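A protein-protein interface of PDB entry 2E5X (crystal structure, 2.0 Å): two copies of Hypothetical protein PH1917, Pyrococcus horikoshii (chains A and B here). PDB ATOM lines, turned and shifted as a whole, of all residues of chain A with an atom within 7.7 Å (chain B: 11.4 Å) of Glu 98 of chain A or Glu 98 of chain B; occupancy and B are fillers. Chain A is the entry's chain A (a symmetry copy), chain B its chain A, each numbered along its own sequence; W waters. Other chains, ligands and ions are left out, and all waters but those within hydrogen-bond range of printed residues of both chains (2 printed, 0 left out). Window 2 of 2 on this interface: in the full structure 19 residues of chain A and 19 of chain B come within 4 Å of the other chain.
NZ of Lys 95 of chain B is in salt-bridge range of OE1 of Glu 98 of chain B (2.8 Å).
The side-chain amino group (NZ) of Lys 95 of chain A lies within salt-bridge range of the side-chain carboxylate (OE1) of Glu 98 of chain A, at 2.8 Å.
Of the printed residues of chain B, Gly 92 of chain A touches Leu 96 (3.5 Å).
No residue of chain B comes within 4 Å of Met 97 of chain A.
Of chain B, only Lys 95 and Glu 98 come within 4 Å of Glu 98 of chain A.
No residue of chain B comes within 4 Å of Gly 99 of chain A.
No residue of chain B comes within 4 Å of Ala 100 of chain A.
Ser 72 of chain B touches none of the printed residues of chain A.
Of the printed residues of chain A, Gly 92 of chain B touches Leu 96 (3.5 Å).
Printed residues of chain A within 4 Å of Lys 95 of chain B: Lys 95 and Glu 98.
Printed residues of chain A within 4 Å of Glu 98 of chain B: Lys 95 and Glu 98.
The nearest printed residue of chain A that does not touch Glu 98 of chain B is Leu 96 of chain A (8.1 Å).
The nearest printed residue of chain B that does not touch Gly 92 of chain A is Leu 73 of chain B (6.9 Å).
Among the printed residues, merely in contact across the chains: Gly 92 of chain A with Leu 96 of chain B (3.5 Å), Lys 95 of chain A with Lys 95 of chain B (3.5 Å), Leu 96 of chain A with Gly 92 of chain B (3.5 Å), Leu 96 of chain A with Leu 96 of chain B (3.8 Å) and Glu 98 of chain A with Glu 98 of chain B (3.97 Å).
Gly 92 of chain A touches Leu 96 of chain B, and with the chains exchanged Leu 96 of chain A touches Gly 92 of chain B.
Lys 95 of chain B touches its own counterpart, Lys 95 of chain A.
Leu 96 of chain A touches its own counterpart, Leu 96 of chain B.
Glu 98 of chain B touches its own counterpart, Glu 98 of chain A.
Of the 7 pairs that touch across the chains among the printed residues, 7 have their exchanged pair printed and touching as well.
Hydrophobic or aromatic side chains of chain A within 4 Å of the printed part of chain B: Leu 96.
Hydrophobic or aromatic side chains of chain B within 4 Å of the printed part of chain A: Leu 96.
Among the printed residues, 7 pairs touch across the chains.
Among the printed residues, Asp or Glu carboxylates within 4 Å of a Lys or Arg side-chain nitrogen of the other chain: Lys 95 of chain A with Glu 98 of chain B (3.3 Å) and Glu 98 of chain A with Lys 95 of chain B (3.3 Å).
NZ of Lys 95 of chain B lies within salt-bridge range of OE1 of Glu 98 of chain A, 3.3 Å away.
The side-chain amino group (NZ) of Lys 95 of chain A is in salt-bridge range of the side-chain carboxylate (OE1) of Glu 98 of chain B, at 3.3 Å.
Water W1 bridges the backbone carbonyl oxygen of Glu 98 of chain A (3.1 Å) and the side-chain amino group of Lys 95 of chain B (3.4 Å).
Water W2 lies within hydrogen-bond range of the backbone carbonyl oxygen (O) of Glu 98 of chain B (3.1 Å) and the side-chain amino group (NZ) of Lys 95 of chain A (3.4 Å).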
ATOM      1  N   SER A  72     -22.812  39.896  24.269  1.00  0.00           N
ATOM      2  CA  SER A  72     -24.021  39.316  23.684  1.00  0.00           C
ATOM      3  C   SER A  72     -24.534  38.095  24.465  1.00  0.00           C
ATOM      4  O   SER A  72     -25.636  37.609  24.255  1.00  0.00           O
ATOM      5  CB  SER A  72     -23.753  38.935  22.219  1.00  0.00           C
ATOM      6  OG  SER A  72     -22.740  37.931  22.146  1.00  0.00           O
ATOM      7  N   LEU A  73     -23.670  37.572  25.364  1.00  0.00           N
ATOM      8  CA  LEU A  73     -24.089  36.439  26.193  1.00  0.00           C
ATOM      9  C   LEU A  73     -24.361  36.866  27.636  1.00  0.00           C
ATOM     10  O   LEU A  73     -24.339  36.067  28.569  1.00  0.00           O
ATOM     11  CB  LEU A  73     -22.964  35.397  26.184  1.00  0.00           C
ATOM     12  CG  LEU A  73     -22.602  34.895  24.786  1.00  0.00           C
ATOM     13  CD1 LEU A  73     -21.552  33.788  24.829  1.00  0.00           C
ATOM     14  CD2 LEU A  73     -23.791  34.316  24.019  1.00  0.00           C
ATOM     15  N   GLU A  91     -15.454  25.939  20.815  1.00  0.00           N
ATOM     16  CA  GLU A  91     -16.454  25.634  19.799  1.00  0.00           C
ATOM     17  C   GLU A  91     -17.830  26.064  20.293  1.00  0.00           C
ATOM     18  O   GLU A  91     -18.645  26.579  19.524  1.00  0.00           O
ATOM     19  CB  GLU A  91     -16.453  24.132  19.493  1.00  0.00           C
ATOM     20  CG  GLU A  91     -15.764  23.765  18.184  1.00  0.00           C
ATOM     21  CD  GLU A  91     -14.324  24.257  18.097  1.00  0.00           C
ATOM     22  OE1 GLU A  91     -13.471  23.764  18.873  1.00  0.00           O
ATOM     23  OE2 GLU A  91     -14.047  25.139  17.246  1.00  0.00           O
ATOM     24  N   GLY A  92     -18.081  25.848  21.582  1.00  0.00           N
ATOM     25  CA  GLY A  92     -19.356  26.233  22.160  1.00  0.00           C
ATOM     26  C   GLY A  92     -19.561  27.735  22.092  1.00  0.00           C
ATOM     27  O   GLY A  92     -20.630  28.209  21.706  1.00  0.00           O
ATOM     28  N   ILE A  93     -18.536  28.489  22.469  1.00  0.00           N
ATOM     29  CA  ILE A  93     -18.614  29.946  22.434  1.00  0.00           C
ATOM     30  C   ILE A  93     -18.889  30.418  21.007  1.00  0.00           C
ATOM     31  O   ILE A  93     -19.769  31.248  20.780  1.00  0.00           O
ATOM     32  CB  ILE A  93     -17.300  30.590  22.926  1.00  0.00           C
ATOM     33  CG1 ILE A  93     -17.028  30.183  24.377  1.00  0.00           C
ATOM     34  CG2 ILE A  93     -17.378  32.109  22.790  1.00  0.00           C
ATOM     35  CD1 ILE A  93     -18.139  30.542  25.347  1.00  0.00           C
ATOM     36  N   LEU A  94     -18.132  29.890  20.049  1.00  0.00           N
ATOM     37  CA  LEU A  94     -18.316  30.266  18.653  1.00  0.00           C
ATOM     38  C   LEU A  94     -19.707  29.894  18.149  1.00  0.00           C
ATOM     39  O   LEU A  94     -20.320  30.649  17.397  1.00  0.00           O
ATOM     40  CB  LEU A  94     -17.246  29.607  17.777  1.00  0.00           C
ATOM     41  CG  LEU A  94     -15.827  30.118  18.037  1.00  0.00           C
ATOM     42  CD1 LEU A  94     -14.838  29.386  17.147  1.00  0.00           C
ATOM     43  CD2 LEU A  94     -15.780  31.619  17.778  1.00  0.00           C
ATOM     44  N   LYS A  95     -20.207  28.734  18.560  1.00  0.00           N
ATOM     45  CA  LYS A  95     -21.538  28.312  18.139  1.00  0.00           C
ATOM     46  C   LYS A  95     -22.579  29.289  18.692  1.00  0.00           C
ATOM     47  O   LYS A  95     -23.486  29.718  17.975  1.00  0.00           O
ATOM     48  CB  LYS A  95     -21.827  26.893  18.631  1.00  0.00           C
ATOM     49  CG  LYS A  95     -23.159  26.325  18.159  1.00  0.00           C
ATOM     50  CD  LYS A  95     -23.226  26.247  16.638  1.00  0.00           C
ATOM     51  CE  LYS A  95     -24.591  25.759  16.157  1.00  0.00           C
ATOM     52  NZ  LYS A  95     -24.689  25.747  14.663  1.00  0.00           N
ATOM     53  N   LEU A  96     -22.443  29.643  19.967  1.00  0.00           N
ATOM     54  CA  LEU A  96     -23.371  30.584  20.591  1.00  0.00           C
ATOM     55  C   LEU A  96     -23.309  31.957  19.920  1.00  0.00           C
ATOM     56  O   LEU A  96     -24.322  32.640  19.811  1.00  0.00           O
ATOM     57  CB  LEU A  96     -23.052  30.749  22.081  1.00  0.00           C
ATOM     58  CG  LEU A  96     -23.464  29.626  23.036  1.00  0.00           C
ATOM     59  CD1 LEU A  96     -22.672  29.732  24.330  1.00  0.00           C
ATOM     60  CD2 LEU A  96     -24.965  29.708  23.300  1.00  0.00           C
ATOM     61  N   MET A  97     -22.119  32.349  19.473  1.00  0.00           N
ATOM     62  CA  MET A  97     -21.911  33.653  18.836  1.00  0.00           C
ATOM     63  C   MET A  97     -22.158  33.629  17.328  1.00  0.00           C
ATOM     64  O   MET A  97     -21.905  34.616  16.635  1.00  0.00           O
ATOM     65  CB  MET A  97     -20.478  34.139  19.093  1.00  0.00           C
ATOM     66  CG  MET A  97     -20.113  34.369  20.562  1.00  0.00           C
ATOM     67  SD  MET A  97     -21.046  35.710  21.298  1.00  0.00           S
ATOM     68  CE  MET A  97     -20.065  37.130  20.740  1.00  0.00           C
ATOM     69  N   GLU A  98     -22.650  32.506  16.826  1.00  0.00           N
ATOM     70  CA  GLU A  98     -22.904  32.354  15.398  1.00  0.00           C
ATOM     71  C   GLU A  98     -23.826  33.434  14.846  1.00  0.00           C
ATOM     72  O   GLU A  98     -24.953  33.594  15.309  1.00  0.00           O
ATOM     73  CB  GLU A  98     -23.505  30.979  15.135  1.00  0.00           C
ATOM     74  CG  GLU A  98     -22.910  30.250  13.958  1.00  0.00           C
ATOM     75  CD  GLU A  98     -23.260  28.777  13.984  1.00  0.00           C
ATOM     76  OE1 GLU A  98     -24.459  28.447  13.862  1.00  0.00           O
ATOM     77  OE2 GLU A  98     -22.333  27.952  14.143  1.00  0.00           O
ATOM     78  N   GLY A  99     -23.336  34.178  13.858  1.00  0.00           N
ATOM     79  CA  GLY A  99     -24.136  35.225  13.248  1.00  0.00           C
ATOM     80  C   GLY A  99     -24.119  36.572  13.949  1.00  0.00           C
ATOM     81  O   GLY A  99     -24.405  37.593  13.323  1.00  0.00           O
ATOM     82  N   ALA A 100     -23.789  36.586  15.237  1.00  0.00           N
ATOM     83  CA  ALA A 100     -23.756  37.832  15.998  1.00  0.00           C
ATOM     84  C   ALA A 100     -22.707  38.802  15.462  1.00  0.00           C
ATOM     85  O   ALA A 100     -21.589  38.404  15.124  1.00  0.00           O
ATOM     86  CB  ALA A 100     -23.490  37.542  17.475  1.00  0.00           C
ATOM     87  N   GLU A 101     -23.076  40.078  15.391  1.00  0.00           N
ATOM     88  CA  GLU A 101     -22.171  41.107  14.901  1.00  0.00           C
ATOM     89  C   GLU A 101     -21.547  41.867  16.069  1.00  0.00           C
ATOM     90  O   GLU A 101     -20.426  42.365  15.964  1.00  0.00           O
ATOM     91  CB  GLU A 101     -22.916  42.076  13.980  1.00  0.00           C
ATOM     92  CG  GLU A 101     -22.000  42.928  13.110  1.00  0.00           C
ATOM     93  CD  GLU A 101     -21.184  42.102  12.122  1.00  0.00           C
ATOM     94  OE1 GLU A 101     -21.323  40.859  12.114  1.00  0.00           O
ATOM     95  OE2 GLU A 101     -20.401  42.702  11.353  1.00  0.00           O
ATOM     96  N   ARG A 103     -19.687  41.500  18.895  1.00  0.00           N
ATOM     97  CA  ARG A 103     -18.853  40.489  19.521  1.00  0.00           C
ATOM     98  C   ARG A 103     -17.954  41.062  20.610  1.00  0.00           C
ATOM     99  O   ARG A 103     -16.914  40.486  20.937  1.00  0.00           O
ATOM    100  CB  ARG A 103     -18.019  39.807  18.436  1.00  0.00           C
ATOM    101  CG  ARG A 103     -18.858  39.349  17.246  1.00  0.00           C
ATOM    102  CD  ARG A 103     -17.993  38.721  16.162  1.00  0.00           C
ATOM    103  NE  ARG A 103     -17.484  37.407  16.542  1.00  0.00           N
ATOM    104  CZ  ARG A 103     -18.218  36.300  16.581  1.00  0.00           C
ATOM    105  NH1 ARG A 103     -19.508  36.340  16.264  1.00  0.00           N
ATOM    106  NH2 ARG A 103     -17.661  35.147  16.920  1.00  0.00           N
ATOM    107  N   ILE B  70     -26.327  18.002  30.468  1.00  0.00           N
ATOM    108  CA  ILE B  70     -26.537  17.582  29.086  1.00  0.00           C
ATOM    109  C   ILE B  70     -25.353  16.820  28.514  1.00  0.00           C
ATOM    110  O   ILE B  70     -24.239  17.338  28.438  1.00  0.00           O
ATOM    111  CB  ILE B  70     -26.857  18.808  28.203  1.00  0.00           C
ATOM    112  CG1 ILE B  70     -28.044  19.566  28.806  1.00  0.00           C
ATOM    113  CG2 ILE B  70     -27.181  18.363  26.774  1.00  0.00           C
ATOM    114  CD1 ILE B  70     -28.382  20.864  28.095  1.00  0.00           C
ATOM    115  N   SER B  72     -24.298  15.785  25.391  1.00  0.00           N
ATOM    116  CA  SER B  72     -23.508  16.312  24.279  1.00  0.00           C
ATOM    117  C   SER B  72     -22.708  17.570  24.658  1.00  0.00           C
ATOM    118  O   SER B  72     -21.838  18.026  23.932  1.00  0.00           O
ATOM    119  CB  SER B  72     -24.431  16.610  23.086  1.00  0.00           C
ATOM    120  OG  SER B  72     -25.377  17.623  23.433  1.00  0.00           O
ATOM    121  N   LEU B  73     -23.063  18.157  25.823  1.00  0.00           N
ATOM    122  CA  LEU B  73     -22.324  19.332  26.294  1.00  0.00           C
ATOM    123  C   LEU B  73     -21.407  18.986  27.468  1.00  0.00           C
ATOM    124  O   LEU B  73     -21.004  19.840  28.255  1.00  0.00           O
ATOM    125  CB  LEU B  73     -23.339  20.388  26.747  1.00  0.00           C
ATOM    126  CG  LEU B  73     -24.316  20.811  25.651  1.00  0.00           C
ATOM    127  CD1 LEU B  73     -25.242  21.934  26.111  1.00  0.00           C
ATOM    128  CD2 LEU B  73     -23.629  21.326  24.386  1.00  0.00           C
ATOM    129  N   PHE B  76     -22.593  20.061  31.010  1.00  0.00           N
ATOM    130  CA  PHE B  76     -22.969  21.470  31.124  1.00  0.00           C
ATOM    131  C   PHE B  76     -24.493  21.564  30.923  1.00  0.00           C
ATOM    132  O   PHE B  76     -25.072  20.769  30.181  1.00  0.00           O
ATOM    133  CB  PHE B  76     -22.192  22.260  30.057  1.00  0.00           C
ATOM    134  CG  PHE B  76     -22.711  23.646  29.784  1.00  0.00           C
ATOM    135  CD1 PHE B  76     -23.858  23.840  29.012  1.00  0.00           C
ATOM    136  CD2 PHE B  76     -22.001  24.765  30.223  1.00  0.00           C
ATOM    137  CE1 PHE B  76     -24.285  25.130  28.674  1.00  0.00           C
ATOM    138  CE2 PHE B  76     -22.416  26.052  29.892  1.00  0.00           C
ATOM    139  CZ  PHE B  76     -23.564  26.238  29.112  1.00  0.00           C
ATOM    140  N   ILE B  88     -27.345  32.881  28.991  1.00  0.00           N
ATOM    141  CA  ILE B  88     -27.662  32.476  27.625  1.00  0.00           C
ATOM    142  C   ILE B  88     -29.088  31.942  27.473  1.00  0.00           C
ATOM    143  O   ILE B  88     -29.600  31.851  26.361  1.00  0.00           O
ATOM    144  CB  ILE B  88     -26.660  31.433  27.095  1.00  0.00           C
ATOM    145  CG1 ILE B  88     -26.784  30.121  27.875  1.00  0.00           C
ATOM    146  CG2 ILE B  88     -25.245  31.990  27.196  1.00  0.00           C
ATOM    147  CD1 ILE B  88     -25.855  29.021  27.370  1.00  0.00           C
ATOM    148  N   GLY B  89     -29.723  31.593  28.591  1.00  0.00           N
ATOM    149  CA  GLY B  89     -31.097  31.102  28.562  1.00  0.00           C
ATOM    150  C   GLY B  89     -31.380  29.815  27.802  1.00  0.00           C
ATOM    151  O   GLY B  89     -30.464  29.109  27.381  1.00  0.00           O
ATOM    152  N   LEU B  90     -32.665  29.506  27.636  1.00  0.00           N
ATOM    153  CA  LEU B  90     -33.071  28.305  26.919  1.00  0.00           C
ATOM    154  C   LEU B  90     -32.633  28.401  25.458  1.00  0.00           C
ATOM    155  O   LEU B  90     -32.310  27.397  24.822  1.00  0.00           O
ATOM    156  CB  LEU B  90     -34.591  28.122  27.002  1.00  0.00           C
ATOM    157  CG  LEU B  90     -35.196  28.089  28.412  1.00  0.00           C
ATOM    158  CD1 LEU B  90     -36.695  27.843  28.313  1.00  0.00           C
ATOM    159  CD2 LEU B  90     -34.528  26.998  29.243  1.00  0.00           C
ATOM    160  N   GLU B  91     -32.621  29.620  24.933  1.00  0.00           N
ATOM    161  CA  GLU B  91     -32.211  29.850  23.553  1.00  0.00           C
ATOM    162  C   GLU B  91     -30.758  29.429  23.375  1.00  0.00           C
ATOM    163  O   GLU B  91     -30.386  28.858  22.347  1.00  0.00           O
ATOM    164  CB  GLU B  91     -32.377  31.331  23.195  1.00  0.00           C
ATOM    165  CG  GLU B  91     -33.601  31.630  22.336  1.00  0.00           C
ATOM    166  CD  GLU B  91     -34.908  31.155  22.956  1.00  0.00           C
ATOM    167  OE1 GLU B  91     -35.310  31.705  24.010  1.00  0.00           O
ATOM    168  OE2 GLU B  91     -35.536  30.229  22.386  1.00  0.00           O
ATOM    169  N   GLY B  92     -29.940  29.717  24.384  1.00  0.00           N
ATOM    170  CA  GLY B  92     -28.537  29.350  24.327  1.00  0.00           C
ATOM    171  C   GLY B  92     -28.365  27.843  24.260  1.00  0.00           C
ATOM    172  O   GLY B  92     -27.591  27.331  23.450  1.00  0.00           O
ATOM    173  N   ILE B  93     -29.086  27.127  25.114  1.00  0.00           N
ATOM    174  CA  ILE B  93     -29.013  25.670  25.132  1.00  0.00           C
ATOM    175  C   ILE B  93     -29.425  25.110  23.771  1.00  0.00           C
ATOM    176  O   ILE B  93     -28.739  24.257  23.211  1.00  0.00           O
ATOM    177  CB  ILE B  93     -29.938  25.075  26.216  1.00  0.00           C
ATOM    178  CG1 ILE B  93     -29.510  25.571  27.601  1.00  0.00           C
ATOM    179  CG2 ILE B  93     -29.911  23.550  26.149  1.00  0.00           C
ATOM    180  CD1 ILE B  93     -28.072  25.254  27.962  1.00  0.00           C
ATOM    181  N   LEU B  94     -30.548  25.592  23.246  1.00  0.00           N
ATOM    182  CA  LEU B  94     -31.028  25.132  21.949  1.00  0.00           C
ATOM    183  C   LEU B  94     -30.036  25.453  20.834  1.00  0.00           C
ATOM    184  O   LEU B  94     -29.831  24.647  19.931  1.00  0.00           O
ATOM    185  CB  LEU B  94     -32.392  25.753  21.632  1.00  0.00           C
ATOM    186  CG  LEU B  94     -33.521  25.279  22.552  1.00  0.00           C
ATOM    187  CD1 LEU B  94     -34.819  25.972  22.181  1.00  0.00           C
ATOM    188  CD2 LEU B  94     -33.660  23.767  22.434  1.00  0.00           C
ATOM    189  N   LYS B  95     -29.420  26.628  20.897  1.00  0.00           N
ATOM    190  CA  LYS B  95     -28.442  27.005  19.882  1.00  0.00           C
ATOM    191  C   LYS B  95     -27.250  26.047  19.946  1.00  0.00           C
ATOM    192  O   LYS B  95     -26.773  25.564  18.916  1.00  0.00           O
ATOM    193  CB  LYS B  95     -27.979  28.446  20.099  1.00  0.00           C
ATOM    194  CG  LYS B  95     -27.027  28.966  19.029  1.00  0.00           C
ATOM    195  CD  LYS B  95     -27.675  28.953  17.650  1.00  0.00           C
ATOM    196  CE  LYS B  95     -26.696  29.391  16.562  1.00  0.00           C
ATOM    197  NZ  LYS B  95     -27.304  29.314  15.196  1.00  0.00           N
ATOM    198  N   LEU B  96     -26.772  25.770  21.156  1.00  0.00           N
ATOM    199  CA  LEU B  96     -25.647  24.855  21.331  1.00  0.00           C
ATOM    200  C   LEU B  96     -25.994  23.446  20.849  1.00  0.00           C
ATOM    201  O   LEU B  96     -25.137  22.743  20.322  1.00  0.00           O
ATOM    202  CB  LEU B  96     -25.235  24.783  22.806  1.00  0.00           C
ATOM    203  CG  LEU B  96     -24.443  25.954  23.392  1.00  0.00           C
ATOM    204  CD1 LEU B  96     -24.542  25.936  24.911  1.00  0.00           C
ATOM    205  CD2 LEU B  96     -22.990  25.866  22.933  1.00  0.00           C
ATOM    206  N   MET B  97     -27.249  23.046  21.030  1.00  0.00           N
ATOM    207  CA  MET B  97     -27.710  21.709  20.641  1.00  0.00           C
ATOM    208  C   MET B  97     -28.193  21.640  19.192  1.00  0.00           C
ATOM    209  O   MET B  97     -28.723  20.619  18.756  1.00  0.00           O
ATOM    210  CB  MET B  97     -28.853  21.260  21.562  1.00  0.00           C
ATOM    211  CG  MET B  97     -28.491  21.122  23.043  1.00  0.00           C
ATOM    212  SD  MET B  97     -27.302  19.814  23.339  1.00  0.00           S
ATOM    213  CE  MET B  97     -28.410  18.379  23.386  1.00  0.00           C
ATOM    214  N   GLU B  98     -28.006  22.725  18.453  1.00  0.00           N
ATOM    215  CA  GLU B  98     -28.447  22.788  17.065  1.00  0.00           C
ATOM    216  C   GLU B  98     -27.871  21.664  16.212  1.00  0.00           C
ATOM    217  O   GLU B  98     -26.655  21.516  16.107  1.00  0.00           O
ATOM    218  CB  GLU B  98     -28.057  24.137  16.472  1.00  0.00           C
ATOM    219  CG  GLU B  98     -29.141  24.803  15.666  1.00  0.00           C
ATOM    220  CD  GLU B  98     -28.841  26.270  15.439  1.00  0.00           C
ATOM    221  OE1 GLU B  98     -27.841  26.575  14.754  1.00  0.00           O
ATOM    222  OE2 GLU B  98     -29.599  27.117  15.961  1.00  0.00           O
ATOM    223  N   GLY B  99     -28.753  20.871  15.611  1.00  0.00           N
ATOM    224  CA  GLY B  99     -28.313  19.778  14.762  1.00  0.00           C
ATOM    225  C   GLY B  99     -27.983  18.475  15.468  1.00  0.00           C
ATOM    226  O   GLY B  99     -28.005  17.415  14.843  1.00  0.00           O
ATOM    227  N   ALA B 100     -27.677  18.541  16.762  1.00  0.00           N
ATOM    228  CA  ALA B 100     -27.334  17.343  17.523  1.00  0.00           C
ATOM    229  C   ALA B 100     -28.497  16.359  17.593  1.00  0.00           C
ATOM    230  O   ALA B 100     -29.651  16.752  17.791  1.00  0.00           O
ATOM    231  CB  ALA B 100     -26.888  17.724  18.934  1.00  0.00           C
ATOM    232  N   GLU B 101     -28.185  15.076  17.434  1.00  0.00           N
ATOM    233  CA  GLU B 101     -29.200  14.033  17.483  1.00  0.00           C
ATOM    234  C   GLU B 101     -29.198  13.352  18.850  1.00  0.00           C
ATOM    235  O   GLU B 101     -30.233  12.865  19.307  1.00  0.00           O
ATOM    236  CB  GLU B 101     -28.954  13.001  16.380  1.00  0.00           C
ATOM    237  CG  GLU B 101     -30.156  12.112  16.088  1.00  0.00           C
ATOM    238  CD  GLU B 101     -31.350  12.890  15.546  1.00  0.00           C
ATOM    239  OE1 GLU B 101     -31.248  14.128  15.400  1.00  0.00           O
ATOM    240  OE2 GLU B 101     -32.391  12.258  15.264  1.00  0.00           O
ATOM    241  N   ASP B 102     -28.036  13.305  19.497  1.00  0.00           N
ATOM    242  CA  ASP B 102     -27.957  12.713  20.826  1.00  0.00           C
ATOM    243  C   ASP B 102     -28.275  13.846  21.788  1.00  0.00           C
ATOM    244  O   ASP B 102     -27.403  14.638  22.154  1.00  0.00           O
ATOM    245  CB  ASP B 102     -26.565  12.151  21.118  1.00  0.00           C
ATOM    246  CG  ASP B 102     -26.474  11.520  22.509  1.00  0.00           C
ATOM    247  OD1 ASP B 102     -27.494  10.955  22.973  1.00  0.00           O
ATOM    248  OD2 ASP B 102     -25.389  11.577  23.134  1.00  0.00           O
ATOM    249  N   ARG B 103     -29.538  13.913  22.189  1.00  0.00           N
ATOM    250  CA  ARG B 103     -30.000  14.971  23.070  1.00  0.00           C
ATOM    251  C   ARG B 103     -30.282  14.476  24.483  1.00  0.00           C
ATOM    252  O   ARG B 103     -31.059  15.085  25.222  1.00  0.00           O
ATOM    253  CB  ARG B 103     -31.253  15.600  22.458  1.00  0.00           C
ATOM    254  CG  ARG B 103     -31.069  15.974  20.990  1.00  0.00           C
ATOM    255  CD  ARG B 103     -32.348  16.550  20.396  1.00  0.00           C
ATOM    256  NE  ARG B 103     -32.641  17.891  20.892  1.00  0.00           N
ATOM    257  CZ  ARG B 103     -31.989  18.988  20.519  1.00  0.00           C
ATOM    258  NH1 ARG B 103     -30.994  18.910  19.643  1.00  0.00           N
ATOM    259  NH2 ARG B 103     -32.342  20.167  21.010  1.00  0.00           N
ATOM    260  N   ILE B 130     -33.359  16.656  25.582  1.00  0.00           N
ATOM    261  CA  ILE B 130     -33.650  18.055  25.305  1.00  0.00           C
ATOM    262  C   ILE B 130     -34.522  18.112  24.055  1.00  0.00           C
ATOM    263  O   ILE B 130     -34.184  17.514  23.035  1.00  0.00           O
ATOM    264  CB  ILE B 130     -32.348  18.848  25.049  1.00  0.00           C
ATOM    265  CG1 ILE B 130     -31.377  18.635  26.221  1.00  0.00           C
ATOM    266  CG2 ILE B 130     -32.663  20.329  24.861  1.00  0.00           C
ATOM    267  CD1 ILE B 130     -31.970  19.001  27.590  1.00  0.00           C
ATOM    268  N   SER B 131     -35.645  18.818  24.142  1.00  0.00           N
ATOM    269  CA  SER B 131     -36.550  18.943  23.004  1.00  0.00           C
ATOM    270  C   SER B 131     -35.946  19.857  21.937  1.00  0.00           C
ATOM    271  O   SER B 131     -34.919  20.499  22.165  1.00  0.00           O
ATOM    272  CB  SER B 131     -37.908  19.490  23.459  1.00  0.00           C
ATOM    273  OG  SER B 131     -37.782  20.788  24.015  1.00  0.00           O
ATOM    274  N   ASN B 132     -36.583  19.908  20.768  1.00  0.00           N
ATOM    275  CA  ASN B 132     -36.098  20.739  19.672  1.00  0.00           C
ATOM    276  C   ASN B 132     -36.526  22.190  19.806  1.00  0.00           C
ATOM    277  O   ASN B 132     -35.928  23.078  19.194  1.00  0.00           O
ATOM    278  CB  ASN B 132     -36.580  20.181  18.332  1.00  0.00           C
ATOM    279  CG  ASN B 132     -35.750  19.011  17.870  1.00  0.00           C
ATOM    280  OD1 ASN B 132     -35.344  18.175  18.673  1.00  0.00           O
ATOM    281  ND2 ASN B 132     -35.494  18.940  16.568  1.00  0.00           N
ATOM    282  N   GLU B 133     -37.560  22.429  20.603  1.00  0.00           N
ATOM    283  CA  GLU B 133     -38.053  23.782  20.815  1.00  0.00           C
ATOM    284  C   GLU B 133     -38.748  23.886  22.165  1.00  0.00           C
ATOM    285  O   GLU B 133     -39.062  22.870  22.782  1.00  0.00           O
ATOM    286  CB  GLU B 133     -39.037  24.168  19.702  1.00  0.00           C
ATOM    287  CG  GLU B 133     -40.345  23.377  19.682  1.00  0.00           C
ATOM    288  CD  GLU B 133     -40.139  21.881  19.469  1.00  0.00           C
ATOM    289  OE1 GLU B 133     -39.969  21.464  18.303  1.00  0.00           O
ATOM    290  OE2 GLU B 133     -40.137  21.128  20.466  1.00  0.00           O
ATOM    291  N   ILE B 145     -37.898  22.747  27.870  1.00  0.00           N
ATOM    292  CA  ILE B 145     -37.084  21.971  26.936  1.00  0.00           C
ATOM    293  C   ILE B 145     -36.600  20.613  27.453  1.00  0.00           C
ATOM    294  O   ILE B 145     -35.689  20.013  26.877  1.00  0.00           O
ATOM    295  CB  ILE B 145     -35.847  22.776  26.452  1.00  0.00           C
ATOM    296  CG1 ILE B 145     -34.896  23.032  27.617  1.00  0.00           C
ATOM    297  CG2 ILE B 145     -36.289  24.105  25.824  1.00  0.00           C
ATOM    298  CD1 ILE B 145     -33.613  23.731  27.200  1.00  0.00           C
HETATM  299  O   HOH W   1     -27.093  32.286  13.533  1.00  0.00           O
HETATM  300  O   HOH W   2     -25.605  22.685  13.467  1.00  0.00           O
